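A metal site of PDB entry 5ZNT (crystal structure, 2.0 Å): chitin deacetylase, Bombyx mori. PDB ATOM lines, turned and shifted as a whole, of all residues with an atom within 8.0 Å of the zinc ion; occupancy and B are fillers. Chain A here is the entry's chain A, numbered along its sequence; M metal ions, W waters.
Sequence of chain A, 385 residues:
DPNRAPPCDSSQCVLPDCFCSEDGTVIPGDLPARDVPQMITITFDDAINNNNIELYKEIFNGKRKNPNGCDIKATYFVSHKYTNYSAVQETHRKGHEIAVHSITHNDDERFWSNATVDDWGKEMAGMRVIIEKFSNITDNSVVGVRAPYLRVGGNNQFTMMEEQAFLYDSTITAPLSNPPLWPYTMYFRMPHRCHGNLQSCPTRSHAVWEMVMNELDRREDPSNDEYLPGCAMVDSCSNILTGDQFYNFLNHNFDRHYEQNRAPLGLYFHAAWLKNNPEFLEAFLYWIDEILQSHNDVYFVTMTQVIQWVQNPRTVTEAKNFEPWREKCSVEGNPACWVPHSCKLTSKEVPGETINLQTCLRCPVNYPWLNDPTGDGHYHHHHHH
Of the 18 residues printed, 3 come within 4 Å of the zinc ion.
N of Asp 46 is in hydrogen-bond range of O of Phe 77.
ND1 of His 105 sits at hydrogen-bond distance from OH of Tyr 149 (3.2 Å).
N of His 101 sits at hydrogen-bond distance from O of Val 78 (2.9 Å).
N of His 105 sits at hydrogen-bond distance from OG of Ser 102 (2.9 Å).
O of Arg 146 is in hydrogen-bond range of ND1 of His 101.
Water W3 lies within hydrogen-bond range of the side-chain carboxylate of Asp 45 (2.8 Å) and a ring nitrogen (NE2) of His 270 (3.0 Å).
Water W2 bridges OD2 of Asp 46 (2.8 Å) and NE2 of His 270 (3.3 Å).
The zinc ion is bound by NE2 of His 105, 2.1 Å away.
A ring nitrogen (NE2) of His 101 is bound to the zinc ion (2.1 Å).
The side-chain carboxylate (OD1) of Asp 46 is bound to the zinc ion (2.1 Å).
The zinc ion is bound by water W2.
Water W3 is bound to the zinc ion, 2.3 Å away.
Water W1 binds the zinc ion, 2.3 Å away.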
ATOM      1  N   PHE A  44     -11.836  -9.241  26.965  1.00  0.00           N
ATOM      2  CA  PHE A  44     -12.964  -9.035  27.872  1.00  0.00           C
ATOM      3  C   PHE A  44     -13.299  -7.558  27.940  1.00  0.00           C
ATOM      4  O   PHE A  44     -12.397  -6.727  28.138  1.00  0.00           O
ATOM      5  CB  PHE A  44     -12.640  -9.565  29.275  1.00  0.00           C
ATOM      6  CG  PHE A  44     -12.351 -11.028  29.298  1.00  0.00           C
ATOM      7  CD1 PHE A  44     -13.388 -11.950  29.245  1.00  0.00           C
ATOM      8  CD2 PHE A  44     -11.041 -11.483  29.330  1.00  0.00           C
ATOM      9  CE1 PHE A  44     -13.118 -13.312  29.238  1.00  0.00           C
ATOM     10  CE2 PHE A  44     -10.765 -12.850  29.330  1.00  0.00           C
ATOM     11  CZ  PHE A  44     -11.813 -13.757  29.297  1.00  0.00           C
ATOM     12  N   ASP A  45     -14.568  -7.229  27.814  1.00  0.00           N
ATOM     13  CA  ASP A  45     -14.944  -5.850  27.917  1.00  0.00           C
ATOM     14  C   ASP A  45     -15.459  -5.582  29.304  1.00  0.00           C
ATOM     15  O   ASP A  45     -15.751  -6.492  30.103  1.00  0.00           O
ATOM     16  CB  ASP A  45     -15.896  -5.465  26.797  1.00  0.00           C
ATOM     17  CG  ASP A  45     -15.231  -5.466  25.439  1.00  0.00           C
ATOM     18  OD1 ASP A  45     -14.043  -5.839  25.349  1.00  0.00           O
ATOM     19  OD2 ASP A  45     -15.913  -5.094  24.445  1.00  0.00           O
ATOM     20  N   ASP A  46     -15.570  -4.284  29.534  1.00  0.00           N
ATOM     21  CA  ASP A  46     -16.273  -3.656  30.625  1.00  0.00           C
ATOM     22  C   ASP A  46     -15.622  -3.989  31.951  1.00  0.00           C
ATOM     23  O   ASP A  46     -14.609  -4.544  31.958  1.00  0.00           O
ATOM     24  CB  ASP A  46     -17.752  -4.096  30.803  1.00  0.00           C
ATOM     25  CG  ASP A  46     -18.635  -4.017  29.540  1.00  0.00           C
ATOM     26  OD1 ASP A  46     -18.218  -3.401  28.589  1.00  0.00           O
ATOM     27  OD2 ASP A  46     -19.754  -4.610  29.613  1.00  0.00           O
ATOM     28  N   ALA A  47     -16.205  -3.569  33.045  1.00  0.00           N
ATOM     29  CA  ALA A  47     -15.554  -3.459  34.337  1.00  0.00           C
ATOM     30  C   ALA A  47     -14.803  -4.683  34.824  1.00  0.00           C
ATOM     31  O   ALA A  47     -15.155  -5.744  34.518  1.00  0.00           O
ATOM     32  CB  ALA A  47     -16.524  -2.956  35.390  1.00  0.00           C
ATOM     33  N   PHE A  77     -10.564  -4.634  27.764  1.00  0.00           N
ATOM     34  CA  PHE A  77     -11.047  -3.315  27.396  1.00  0.00           C
ATOM     35  C   PHE A  77     -11.902  -2.804  28.554  1.00  0.00           C
ATOM     36  O   PHE A  77     -13.058  -3.212  28.716  1.00  0.00           O
ATOM     37  CB  PHE A  77     -11.823  -3.354  26.078  1.00  0.00           C
ATOM     38  CG  PHE A  77     -10.931  -3.614  24.880  1.00  0.00           C
ATOM     39  CD1 PHE A  77     -10.212  -2.577  24.300  1.00  0.00           C
ATOM     40  CD2 PHE A  77     -10.798  -4.899  24.377  1.00  0.00           C
ATOM     41  CE1 PHE A  77      -9.368  -2.825  23.223  1.00  0.00           C
ATOM     42  CE2 PHE A  77      -9.974  -5.138  23.292  1.00  0.00           C
ATOM     43  CZ  PHE A  77      -9.260  -4.116  22.721  1.00  0.00           C
ATOM     44  N   VAL A  78     -11.328  -1.925  29.358  1.00  0.00           N
ATOM     45  CA  VAL A  78     -11.860  -1.627  30.692  1.00  0.00           C
ATOM     46  C   VAL A  78     -12.671  -0.348  30.617  1.00  0.00           C
ATOM     47  O   VAL A  78     -12.186   0.665  30.105  1.00  0.00           O
ATOM     48  CB  VAL A  78     -10.714  -1.488  31.711  1.00  0.00           C
ATOM     49  CG1 VAL A  78     -11.280  -1.141  33.106  1.00  0.00           C
ATOM     50  CG2 VAL A  78      -9.921  -2.824  31.773  1.00  0.00           C
ATOM     51  N   SER A  79     -13.900  -0.396  31.142  1.00  0.00           N
ATOM     52  CA  SER A  79     -14.712   0.793  31.342  1.00  0.00           C
ATOM     53  C   SER A  79     -14.653   1.184  32.826  1.00  0.00           C
ATOM     54  O   SER A  79     -14.406   0.345  33.686  1.00  0.00           O
ATOM     55  CB  SER A  79     -16.173   0.546  30.910  1.00  0.00           C
ATOM     56  OG  SER A  79     -16.730  -0.561  31.633  1.00  0.00           O
ATOM     57  N   HIS A 101     -12.099   1.355  27.325  1.00  0.00           N
ATOM     58  CA  HIS A 101     -13.451   1.096  26.855  1.00  0.00           C
ATOM     59  C   HIS A 101     -14.376   2.235  27.316  1.00  0.00           C
ATOM     60  O   HIS A 101     -15.572   2.019  27.532  1.00  0.00           O
ATOM     61  CB  HIS A 101     -13.924  -0.262  27.360  1.00  0.00           C
ATOM     62  CG  HIS A 101     -15.183  -0.783  26.716  1.00  0.00           C
ATOM     63  ND1 HIS A 101     -15.411  -0.739  25.356  1.00  0.00           N
ATOM     64  CD2 HIS A 101     -16.249  -1.418  27.261  1.00  0.00           C
ATOM     65  CE1 HIS A 101     -16.573  -1.302  25.090  1.00  0.00           C
ATOM     66  NE2 HIS A 101     -17.104  -1.724  26.227  1.00  0.00           N
ATOM     67  N   SER A 102     -13.801   3.425  27.535  1.00  0.00           N
ATOM     68  CA  SER A 102     -14.452   4.706  27.878  1.00  0.00           C
ATOM     69  C   SER A 102     -14.727   4.885  29.375  1.00  0.00           C
ATOM     70  O   SER A 102     -14.713   3.930  30.161  1.00  0.00           O
ATOM     71  CB  SER A 102     -15.761   4.921  27.098  1.00  0.00           C
ATOM     72  OG  SER A 102     -16.846   4.343  27.773  1.00  0.00           O
ATOM     73  N   HIS A 105     -19.272   4.651  29.266  1.00  0.00           N
ATOM     74  CA  HIS A 105     -19.994   3.582  28.560  1.00  0.00           C
ATOM     75  C   HIS A 105     -21.416   4.020  28.208  1.00  0.00           C
ATOM     76  O   HIS A 105     -22.376   3.256  28.326  1.00  0.00           O
ATOM     77  CB  HIS A 105     -20.007   2.290  29.390  1.00  0.00           C
ATOM     78  CG  HIS A 105     -20.081   1.039  28.563  1.00  0.00           C
ATOM     79  ND1 HIS A 105     -21.258   0.561  28.016  1.00  0.00           N
ATOM     80  CD2 HIS A 105     -19.116   0.159  28.183  1.00  0.00           C
ATOM     81  CE1 HIS A 105     -21.028  -0.561  27.361  1.00  0.00           C
ATOM     82  NE2 HIS A 105     -19.723  -0.814  27.426  1.00  0.00           N
ATOM     83  N   ARG A 146     -11.454   0.383  22.488  1.00  0.00           N
ATOM     84  CA  ARG A 146     -12.648  -0.223  21.906  1.00  0.00           C
ATOM     85  C   ARG A 146     -13.854   0.588  22.356  1.00  0.00           C
ATOM     86  O   ARG A 146     -14.047   0.783  23.564  1.00  0.00           O
ATOM     87  CB  ARG A 146     -12.806  -1.682  22.320  1.00  0.00           C
ATOM     88  CG  ARG A 146     -14.113  -2.328  21.816  1.00  0.00           C
ATOM     89  CD  ARG A 146     -14.083  -3.859  22.056  1.00  0.00           C
ATOM     90  NE  ARG A 146     -13.180  -4.572  21.141  1.00  0.00           N
ATOM     91  CZ  ARG A 146     -12.802  -5.845  21.288  1.00  0.00           C
ATOM     92  NH1 ARG A 146     -13.233  -6.557  22.327  1.00  0.00           N
ATOM     93  NH2 ARG A 146     -11.995  -6.386  20.382  1.00  0.00           N
ATOM     94  N   ALA A 147     -14.664   1.035  21.401  1.00  0.00           N
ATOM     95  CA  ALA A 147     -15.820   1.884  21.720  1.00  0.00           C
ATOM     96  C   ALA A 147     -16.977   1.051  22.255  1.00  0.00           C
ATOM     97  O   ALA A 147     -17.218  -0.067  21.789  1.00  0.00           O
ATOM     98  CB  ALA A 147     -16.284   2.663  20.477  1.00  0.00           C
ATOM     99  N   PRO A 148     -17.704   1.582  23.251  1.00  0.00           N
ATOM    100  CA  PRO A 148     -18.954   0.953  23.683  1.00  0.00           C
ATOM    101  C   PRO A 148     -19.890   0.672  22.526  1.00  0.00           C
ATOM    102  O   PRO A 148     -19.986   1.452  21.561  1.00  0.00           O
ATOM    103  CB  PRO A 148     -19.549   1.993  24.645  1.00  0.00           C
ATOM    104  CG  PRO A 148     -18.333   2.670  25.232  1.00  0.00           C
ATOM    105  CD  PRO A 148     -17.359   2.770  24.050  1.00  0.00           C
ATOM    106  N   TYR A 149     -20.563  -0.482  22.617  1.00  0.00           N
ATOM    107  CA  TYR A 149     -21.510  -0.999  21.621  1.00  0.00           C
ATOM    108  C   TYR A 149     -20.884  -1.084  20.220  1.00  0.00           C
ATOM    109  O   TYR A 149     -21.612  -1.142  19.217  1.00  0.00           O
ATOM    110  CB  TYR A 149     -22.823  -0.186  21.659  1.00  0.00           C
ATOM    111  CG  TYR A 149     -23.270   0.003  23.095  1.00  0.00           C
ATOM    112  CD1 TYR A 149     -23.950  -1.005  23.782  1.00  0.00           C
ATOM    113  CD2 TYR A 149     -22.918   1.148  23.814  1.00  0.00           C
ATOM    114  CE1 TYR A 149     -24.313  -0.852  25.125  1.00  0.00           C
ATOM    115  CE2 TYR A 149     -23.260   1.301  25.170  1.00  0.00           C
ATOM    116  CZ  TYR A 149     -23.950   0.296  25.809  1.00  0.00           C
ATOM    117  OH  TYR A 149     -24.297   0.448  27.123  1.00  0.00           O
ATOM    118  N   LEU A 150     -19.554  -1.122  20.140  1.00  0.00           N
ATOM    119  CA  LEU A 150     -18.798  -1.165  18.883  1.00  0.00           C
ATOM    120  C   LEU A 150     -19.252  -0.059  17.927  1.00  0.00           C
ATOM    121  O   LEU A 150     -19.356  -0.252  16.723  1.00  0.00           O
ATOM    122  CB  LEU A 150     -18.909  -2.547  18.227  1.00  0.00           C
ATOM    123  CG  LEU A 150     -18.472  -3.746  19.101  1.00  0.00           C
ATOM    124  CD1 LEU A 150     -18.545  -5.054  18.319  1.00  0.00           C
ATOM    125  CD2 LEU A 150     -17.029  -3.547  19.571  1.00  0.00           C
ATOM    126  N   MET A 233     -18.903 -10.110  18.700  1.00  0.00           N
ATOM    127  CA  MET A 233     -18.896 -10.465  20.115  1.00  0.00           C
ATOM    128  C   MET A 233     -19.478 -11.857  20.285  1.00  0.00           C
ATOM    129  O   MET A 233     -20.542 -12.165  19.726  1.00  0.00           O
ATOM    130  CB  MET A 233     -19.693  -9.459  20.936  1.00  0.00           C
ATOM    131  CG  MET A 233     -19.241  -8.005  20.783  1.00  0.00           C
ATOM    132  SD  MET A 233     -17.518  -7.758  21.298  1.00  0.00           S
ATOM    133  CE  MET A 233     -17.624  -8.296  23.011  1.00  0.00           C
ATOM    134  N   PHE A 269     -15.164 -11.521  24.566  1.00  0.00           N
ATOM    135  CA  PHE A 269     -16.123 -11.934  25.582  1.00  0.00           C
ATOM    136  C   PHE A 269     -16.581 -10.782  26.472  1.00  0.00           C
ATOM    137  O   PHE A 269     -15.913  -9.760  26.628  1.00  0.00           O
ATOM    138  CB  PHE A 269     -15.545 -13.004  26.510  1.00  0.00           C
ATOM    139  CG  PHE A 269     -15.270 -14.318  25.842  1.00  0.00           C
ATOM    140  CD1 PHE A 269     -16.274 -15.253  25.680  1.00  0.00           C
ATOM    141  CD2 PHE A 269     -13.995 -14.628  25.389  1.00  0.00           C
ATOM    142  CE1 PHE A 269     -16.009 -16.491  25.075  1.00  0.00           C
ATOM    143  CE2 PHE A 269     -13.716 -15.851  24.770  1.00  0.00           C
ATOM    144  CZ  PHE A 269     -14.724 -16.773  24.605  1.00  0.00           C
ATOM    145  N   HIS A 270     -17.739 -11.012  27.089  1.00  0.00           N
ATOM    146  CA  HIS A 270     -18.106 -10.386  28.364  1.00  0.00           C
ATOM    147  C   HIS A 270     -18.011 -11.456  29.429  1.00  0.00           C
ATOM    148  O   HIS A 270     -18.565 -12.545  29.251  1.00  0.00           O
ATOM    149  CB  HIS A 270     -19.515  -9.817  28.346  1.00  0.00           C
ATOM    150  CG  HIS A 270     -19.690  -8.706  27.360  1.00  0.00           C
ATOM    151  ND1 HIS A 270     -20.042  -8.929  26.055  1.00  0.00           N
ATOM    152  CD2 HIS A 270     -19.537  -7.367  27.497  1.00  0.00           C
ATOM    153  CE1 HIS A 270     -20.120  -7.767  25.425  1.00  0.00           C
ATOM    154  NE2 HIS A 270     -19.820  -6.809  26.272  1.00  0.00           N
HETATM  155 ZN    ZN M   1     -18.944  -2.630  26.742  1.00  0.00          ZN
HETATM  156  O   HOH W   1     -19.721  -2.346  24.584  1.00  0.00           O
HETATM  157  O   HOH W   2     -20.738  -3.746  27.143  1.00  0.00           O
HETATM  158  O   HOH W   3     -18.496  -4.298  25.225  1.00  0.00           O
